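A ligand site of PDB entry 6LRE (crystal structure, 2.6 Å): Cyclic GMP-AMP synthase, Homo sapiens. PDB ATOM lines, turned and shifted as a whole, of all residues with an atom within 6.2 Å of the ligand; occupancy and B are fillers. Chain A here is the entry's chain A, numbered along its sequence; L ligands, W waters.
OG of Ser 278 sits at hydrogen-bond distance from O4 of the ligand, 2.7 Å away. The side-chain amide nitrogen (ND2) of Asn 326 lies within hydrogen-bond range of an oxygen (O2) of the ligand, 3.1 Å away. The side-chain hydroxyl (OH) of Tyr 280 lies close to a nitrogen (N1) of the ligand (3.4 Å).
The side-chain hydroxyl (OG) of Ser 278 lies close to the backbone NH (N) of Tyr 280. ND1 of His 281 lies within hydrogen-bond range of N of Ser 278 (3.0 Å). N of Asn 326 is in hydrogen-bond range of O of Phe 332, 2.8 Å away. The side-chain amide oxygen (OD1) of Asn 326 lies within hydrogen-bond range of the backbone NH (N) of Ile 329 (2.8 Å). The side-chain carboxylate (OE2) of Glu 227 sits at hydrogen-bond distance from the side-chain hydroxyl (OH) of Tyr 280, at 2.9 Å.
Residues that only touch the ligand: Arg 220 (3.3 Å), His 281 (3.5 Å), Phe 332 (3.4 Å) and Leu 334 (3.5 Å). Hydrophobic or aromatic side chains within 4 Å of the ligand: Tyr 280, His 281, Phe 332 and Leu 334. Of the 20 residues printed, 7 come within 4 Å of the ligand.
Water W1 lies within hydrogen-bond range of O1 of the ligand, OE2 of Glu 227, N of Phe 223 and OH of Tyr 280. Water W2 lies within hydrogen-bond range of an oxygen (O5) of the ligand (2.7 Å), the side-chain hydroxyl (OG) of Ser 279 (2.9 Å) and the backbone NH (N) of Tyr 280 (3.2 Å). Water W4 lies within hydrogen-bond range of N1 of the ligand (2.9 Å), O of Leu 221 (3.0 Å) and ND2 of Asn 326 (3.3 Å). Water W3 lies within hydrogen-bond range of NE of Arg 220, O of Leu 221 and N1 of the ligand.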
ATOM      1  N   ALA A  91      11.135  10.772  30.999  1.00  0.00           N
ATOM      2  CA  ALA A  91      10.232  10.389  29.922  1.00  0.00           C
ATOM      3  C   ALA A  91      10.939   9.769  28.733  1.00  0.00           C
ATOM      4  O   ALA A  91      10.336   8.955  28.030  1.00  0.00           O
ATOM      5  CB  ALA A  91       9.431  11.603  29.440  1.00  0.00           C
ATOM      6  N   TYR A  92      12.203  10.126  28.486  1.00  0.00           N
ATOM      7  CA  TYR A  92      12.954   9.687  27.331  1.00  0.00           C
ATOM      8  C   TYR A  92      13.870   8.524  27.699  1.00  0.00           C
ATOM      9  O   TYR A  92      14.422   8.486  28.802  1.00  0.00           O
ATOM     10  CB  TYR A  92      13.762  10.844  26.746  1.00  0.00           C
ATOM     11  CG  TYR A  92      12.924  12.055  26.396  1.00  0.00           C
ATOM     12  CD1 TYR A  92      12.546  12.981  27.364  1.00  0.00           C
ATOM     13  CD2 TYR A  92      12.487  12.258  25.087  1.00  0.00           C
ATOM     14  CE1 TYR A  92      11.768  14.074  27.047  1.00  0.00           C
ATOM     15  CE2 TYR A  92      11.709  13.351  24.770  1.00  0.00           C
ATOM     16  CZ  TYR A  92      11.354  14.259  25.744  1.00  0.00           C
ATOM     17  OH  TYR A  92      10.574  15.344  25.415  1.00  0.00           O
ATOM     18  N   PRO A 150       5.396  12.368  15.622  1.00  0.00           N
ATOM     19  CA  PRO A 150       4.779  12.255  14.289  1.00  0.00           C
ATOM     20  C   PRO A 150       5.828  12.187  13.188  1.00  0.00           C
ATOM     21  O   PRO A 150       6.690  13.056  13.118  1.00  0.00           O
ATOM     22  CB  PRO A 150       3.929  13.533  14.175  1.00  0.00           C
ATOM     23  CG  PRO A 150       3.955  14.168  15.546  1.00  0.00           C
ATOM     24  CD  PRO A 150       5.221  13.713  16.190  1.00  0.00           C
ATOM     25  N   LYS A 206      11.291  10.344  19.856  1.00  0.00           N
ATOM     26  CA  LYS A 206      11.222  11.752  20.253  1.00  0.00           C
ATOM     27  C   LYS A 206      12.616  12.264  20.567  1.00  0.00           C
ATOM     28  O   LYS A 206      13.346  11.646  21.337  1.00  0.00           O
ATOM     29  CB  LYS A 206      10.309  11.931  21.465  1.00  0.00           C
ATOM     30  CG  LYS A 206       9.757  13.342  21.612  1.00  0.00           C
ATOM     31  CD  LYS A 206       8.824  13.690  20.470  1.00  0.00           C
ATOM     32  CE  LYS A 206       8.811  15.187  20.203  1.00  0.00           C
ATOM     33  NZ  LYS A 206       7.500  15.630  19.656  1.00  0.00           N
ATOM     34  N   ARG A 220      10.263   8.564  23.921  1.00  0.00           N
ATOM     35  CA  ARG A 220       9.503   9.116  25.029  1.00  0.00           C
ATOM     36  C   ARG A 220       8.335   8.203  25.380  1.00  0.00           C
ATOM     37  O   ARG A 220       7.742   7.559  24.507  1.00  0.00           O
ATOM     38  CB  ARG A 220       8.973  10.520  24.696  1.00  0.00           C
ATOM     39  CG  ARG A 220       8.732  11.374  25.935  1.00  0.00           C
ATOM     40  CD  ARG A 220       8.042  12.695  25.599  1.00  0.00           C
ATOM     41  NE  ARG A 220       7.083  12.560  24.505  1.00  0.00           N
ATOM     42  CZ  ARG A 220       6.734  13.562  23.694  1.00  0.00           C
ATOM     43  NH1 ARG A 220       7.297  14.759  23.841  1.00  0.00           N
ATOM     44  NH2 ARG A 220       5.849  13.355  22.736  1.00  0.00           N
ATOM     45  N   LEU A 221       8.033   8.145  26.678  1.00  0.00           N
ATOM     46  CA  LEU A 221       6.905   7.349  27.149  1.00  0.00           C
ATOM     47  C   LEU A 221       5.597   7.900  26.606  1.00  0.00           C
ATOM     48  O   LEU A 221       5.394   9.112  26.523  1.00  0.00           O
ATOM     49  CB  LEU A 221       6.857   7.323  28.673  1.00  0.00           C
ATOM     50  CG  LEU A 221       7.970   6.506  29.336  1.00  0.00           C
ATOM     51  CD1 LEU A 221       7.737   6.428  30.833  1.00  0.00           C
ATOM     52  CD2 LEU A 221       8.038   5.115  28.720  1.00  0.00           C
ATOM     53  N   SER A 222       4.691   6.993  26.225  1.00  0.00           N
ATOM     54  CA  SER A 222       3.396   7.359  25.674  1.00  0.00           C
ATOM     55  C   SER A 222       2.325   6.511  26.333  1.00  0.00           C
ATOM     56  O   SER A 222       2.504   5.304  26.496  1.00  0.00           O
ATOM     57  CB  SER A 222       3.373   7.181  24.157  1.00  0.00           C
ATOM     58  OG  SER A 222       2.203   7.753  23.594  1.00  0.00           O
ATOM     59  N   PHE A 223       1.222   7.150  26.718  1.00  0.00           N
ATOM     60  CA  PHE A 223       0.083   6.499  27.337  1.00  0.00           C
ATOM     61  C   PHE A 223      -1.200   6.987  26.692  1.00  0.00           C
ATOM     62  O   PHE A 223      -2.236   7.148  27.353  1.00  0.00           O
ATOM     63  CB  PHE A 223       0.059   6.734  28.852  1.00  0.00           C
ATOM     64  CG  PHE A 223       1.311   6.306  29.542  1.00  0.00           C
ATOM     65  CD1 PHE A 223       2.405   7.144  29.623  1.00  0.00           C
ATOM     66  CD2 PHE A 223       1.396   5.050  30.125  1.00  0.00           C
ATOM     67  CE1 PHE A 223       3.557   6.750  30.269  1.00  0.00           C
ATOM     68  CE2 PHE A 223       2.554   4.649  30.765  1.00  0.00           C
ATOM     69  CZ  PHE A 223       3.630   5.498  30.834  1.00  0.00           C
ATOM     70  N   SER A 224      -1.138   7.249  25.396  1.00  0.00           N
ATOM     71  CA  SER A 224      -2.327   7.701  24.667  1.00  0.00           C
ATOM     72  C   SER A 224      -3.485   6.714  24.806  1.00  0.00           C
ATOM     73  O   SER A 224      -4.635   7.128  24.737  1.00  0.00           O
ATOM     74  CB  SER A 224      -1.978   7.928  23.200  1.00  0.00           C
ATOM     75  OG  SER A 224      -2.306   6.790  22.412  1.00  0.00           O
ATOM     76  N   GLU A 227      -4.836   7.394  28.418  1.00  0.00           N
ATOM     77  CA  GLU A 227      -5.545   8.667  28.320  1.00  0.00           C
ATOM     78  C   GLU A 227      -6.917   8.481  27.683  1.00  0.00           C
ATOM     79  O   GLU A 227      -7.909   9.061  28.153  1.00  0.00           O
ATOM     80  CB  GLU A 227      -4.703   9.675  27.525  1.00  0.00           C
ATOM     81  CG  GLU A 227      -3.472  10.176  28.257  1.00  0.00           C
ATOM     82  CD  GLU A 227      -2.332  10.542  27.319  1.00  0.00           C
ATOM     83  OE1 GLU A 227      -2.604  10.875  26.144  1.00  0.00           O
ATOM     84  OE2 GLU A 227      -1.155  10.513  27.763  1.00  0.00           O
ATOM     85  N   LYS A 276       4.867  26.316  20.726  1.00  0.00           N
ATOM     86  CA  LYS A 276       5.166  25.053  21.396  1.00  0.00           C
ATOM     87  C   LYS A 276       4.040  24.560  22.296  1.00  0.00           C
ATOM     88  O   LYS A 276       4.137  23.447  22.813  1.00  0.00           O
ATOM     89  CB  LYS A 276       6.468  25.166  22.194  1.00  0.00           C
ATOM     90  CG  LYS A 276       7.722  25.380  21.325  1.00  0.00           C
ATOM     91  CD  LYS A 276       7.771  24.403  20.135  1.00  0.00           C
ATOM     92  CE  LYS A 276       7.798  22.940  20.575  1.00  0.00           C
ATOM     93  NZ  LYS A 276       6.877  22.094  19.765  1.00  0.00           N
ATOM     94  N   PHE A 277       2.977  25.344  22.478  1.00  0.00           N
ATOM     95  CA  PHE A 277       1.823  24.865  23.209  1.00  0.00           C
ATOM     96  C   PHE A 277       0.988  23.959  22.316  1.00  0.00           C
ATOM     97  O   PHE A 277       0.791  24.246  21.122  1.00  0.00           O
ATOM     98  CB  PHE A 277       0.968  26.026  23.715  1.00  0.00           C
ATOM     99  CG  PHE A 277       1.670  26.892  24.726  1.00  0.00           C
ATOM    100  CD1 PHE A 277       1.910  26.427  26.006  1.00  0.00           C
ATOM    101  CD2 PHE A 277       2.096  28.164  24.383  1.00  0.00           C
ATOM    102  CE1 PHE A 277       2.561  27.211  26.936  1.00  0.00           C
ATOM    103  CE2 PHE A 277       2.754  28.963  25.302  1.00  0.00           C
ATOM    104  CZ  PHE A 277       2.980  28.482  26.587  1.00  0.00           C
ATOM    105  N   SER A 278       0.504  22.853  22.881  1.00  0.00           N
ATOM    106  CA  SER A 278      -0.238  21.864  22.118  1.00  0.00           C
ATOM    107  C   SER A 278      -1.452  21.412  22.923  1.00  0.00           C
ATOM    108  O   SER A 278      -1.550  21.644  24.135  1.00  0.00           O
ATOM    109  CB  SER A 278       0.639  20.673  21.741  1.00  0.00           C
ATOM    110  OG  SER A 278       0.790  19.775  22.840  1.00  0.00           O
ATOM    111  N   SER A 279      -2.372  20.740  22.237  1.00  0.00           N
ATOM    112  CA  SER A 279      -3.546  20.199  22.911  1.00  0.00           C
ATOM    113  C   SER A 279      -3.192  19.175  23.972  1.00  0.00           C
ATOM    114  O   SER A 279      -4.026  18.893  24.837  1.00  0.00           O
ATOM    115  CB  SER A 279      -4.516  19.605  21.888  1.00  0.00           C
ATOM    116  OG  SER A 279      -3.992  18.403  21.362  1.00  0.00           O
ATOM    117  N   TYR A 280      -1.966  18.635  23.952  1.00  0.00           N
ATOM    118  CA  TYR A 280      -1.575  17.710  25.007  1.00  0.00           C
ATOM    119  C   TYR A 280      -1.308  18.432  26.325  1.00  0.00           C
ATOM    120  O   TYR A 280      -1.535  17.873  27.408  1.00  0.00           O
ATOM    121  CB  TYR A 280      -0.340  16.898  24.604  1.00  0.00           C
ATOM    122  CG  TYR A 280      -0.048  15.784  25.584  1.00  0.00           C
ATOM    123  CD1 TYR A 280      -0.798  14.601  25.547  1.00  0.00           C
ATOM    124  CD2 TYR A 280       0.927  15.912  26.574  1.00  0.00           C
ATOM    125  CE1 TYR A 280      -0.552  13.578  26.448  1.00  0.00           C
ATOM    126  CE2 TYR A 280       1.168  14.895  27.482  1.00  0.00           C
ATOM    127  CZ  TYR A 280       0.417  13.726  27.410  1.00  0.00           C
ATOM    128  OH  TYR A 280       0.651  12.708  28.293  1.00  0.00           O
ATOM    129  N   HIS A 281      -0.800  19.667  26.251  1.00  0.00           N
ATOM    130  CA  HIS A 281      -0.665  20.452  27.478  1.00  0.00           C
ATOM    131  C   HIS A 281      -2.021  20.725  28.099  1.00  0.00           C
ATOM    132  O   HIS A 281      -2.211  20.555  29.310  1.00  0.00           O
ATOM    133  CB  HIS A 281       0.058  21.774  27.183  1.00  0.00           C
ATOM    134  CG  HIS A 281       1.469  21.598  26.683  1.00  0.00           C
ATOM    135  ND1 HIS A 281       1.854  21.978  25.417  1.00  0.00           N
ATOM    136  CD2 HIS A 281       2.580  21.110  27.289  1.00  0.00           C
ATOM    137  CE1 HIS A 281       3.138  21.717  25.256  1.00  0.00           C
ATOM    138  NE2 HIS A 281       3.601  21.184  26.375  1.00  0.00           N
ATOM    139  N   ASN A 326       3.710  15.933  33.851  1.00  0.00           N
ATOM    140  CA  ASN A 326       3.085  14.856  33.088  1.00  0.00           C
ATOM    141  C   ASN A 326       2.252  14.003  34.020  1.00  0.00           C
ATOM    142  O   ASN A 326       2.694  13.610  35.102  1.00  0.00           O
ATOM    143  CB  ASN A 326       4.156  14.005  32.393  1.00  0.00           C
ATOM    144  CG  ASN A 326       3.555  12.867  31.580  1.00  0.00           C
ATOM    145  OD1 ASN A 326       3.082  11.870  32.137  1.00  0.00           O
ATOM    146  ND2 ASN A 326       3.598  12.996  30.256  1.00  0.00           N
ATOM    147  N   ILE A 329       4.186  10.799  34.427  1.00  0.00           N
ATOM    148  CA  ILE A 329       5.560  10.974  34.880  1.00  0.00           C
ATOM    149  C   ILE A 329       5.651  12.280  35.658  1.00  0.00           C
ATOM    150  O   ILE A 329       5.968  13.323  35.079  1.00  0.00           O
ATOM    151  CB  ILE A 329       6.529  10.984  33.683  1.00  0.00           C
ATOM    152  CG1 ILE A 329       6.256   9.782  32.770  1.00  0.00           C
ATOM    153  CG2 ILE A 329       7.964  10.962  34.169  1.00  0.00           C
ATOM    154  CD1 ILE A 329       6.436  10.081  31.291  1.00  0.00           C
ATOM    155  N   PHE A 332       8.457  14.920  35.332  1.00  0.00           N
ATOM    156  CA  PHE A 332       8.633  15.480  34.000  1.00  0.00           C
ATOM    157  C   PHE A 332       7.711  16.690  33.879  1.00  0.00           C
ATOM    158  O   PHE A 332       6.480  16.532  33.834  1.00  0.00           O
ATOM    159  CB  PHE A 332       8.338  14.408  32.951  1.00  0.00           C
ATOM    160  CG  PHE A 332       8.494  14.869  31.533  1.00  0.00           C
ATOM    161  CD1 PHE A 332       9.485  15.775  31.183  1.00  0.00           C
ATOM    162  CD2 PHE A 332       7.658  14.369  30.547  1.00  0.00           C
ATOM    163  CE1 PHE A 332       9.624  16.178  29.869  1.00  0.00           C
ATOM    164  CE2 PHE A 332       7.796  14.773  29.233  1.00  0.00           C
ATOM    165  CZ  PHE A 332       8.773  15.684  28.900  1.00  0.00           C
ATOM    166  N   LEU A 334       6.241  19.525  31.809  1.00  0.00           N
ATOM    167  CA  LEU A 334       6.032  20.008  30.450  1.00  0.00           C
ATOM    168  C   LEU A 334       6.158  21.523  30.313  1.00  0.00           C
ATOM    169  O   LEU A 334       6.221  22.026  29.192  1.00  0.00           O
ATOM    170  CB  LEU A 334       4.659  19.553  29.944  1.00  0.00           C
ATOM    171  CG  LEU A 334       4.284  18.084  30.130  1.00  0.00           C
ATOM    172  CD1 LEU A 334       2.818  17.840  29.798  1.00  0.00           C
ATOM    173  CD2 LEU A 334       5.181  17.181  29.293  1.00  0.00           C
HETATM  174  C1  LIG L   1       2.651  13.822  24.272  1.00  0.00           C
HETATM  175  C2  LIG L   1       4.408  18.468  23.121  1.00  0.00           C
HETATM  176  C3  LIG L   1       3.453  14.960  24.519  1.00  0.00           C
HETATM  177  C4  LIG L   1       3.433  16.063  23.617  1.00  0.00           C
HETATM  178  C5  LIG L   1       2.668  12.698  25.215  1.00  0.00           C
HETATM  179  C6  LIG L   1       4.262  14.986  25.668  1.00  0.00           C
HETATM  180  C7  LIG L   1       5.059  16.074  25.933  1.00  0.00           C
HETATM  181  C8  LIG L   1       5.061  17.174  25.055  1.00  0.00           C
HETATM  182  C9  LIG L   1       4.276  17.195  23.929  1.00  0.00           C
HETATM  183  C10 LIG L   1       4.280  13.840  26.582  1.00  0.00           C
HETATM  184  C11 LIG L   1       2.432  17.008  21.372  1.00  0.00           C
HETATM  185  N1  LIG L   1       3.475  12.752  26.329  1.00  0.00           N
HETATM  186  C12 LIG L   1       1.839  13.775  23.163  1.00  0.00           C
HETATM  187  C13 LIG L   1       2.582  15.966  22.456  1.00  0.00           C
HETATM  188  C14 LIG L   1       1.814  14.841  22.261  1.00  0.00           C
HETATM  189  O1  LIG L   1       1.982  11.709  25.032  1.00  0.00           O
HETATM  190  O2  LIG L   1       4.978  13.838  27.585  1.00  0.00           O
HETATM  191  O3  LIG L   1       3.458  17.340  20.743  1.00  0.00           O
HETATM  192  O4  LIG L   1       3.380  19.128  22.919  1.00  0.00           O
HETATM  193  O5  LIG L   1       1.279  17.440  21.153  1.00  0.00           O
HETATM  194  O6  LIG L   1       5.547  18.780  22.715  1.00  0.00           O
HETATM  195  O   HOH W   1       1.372  10.010  26.619  1.00  0.00           O
HETATM  196  O   HOH W   2      -1.421  17.181  21.132  1.00  0.00           O
HETATM  197  O   HOH W   3       5.141  10.913  24.494  1.00  0.00           O
HETATM  198  O   HOH W   4       3.386  10.476  28.200  1.00  0.00           O
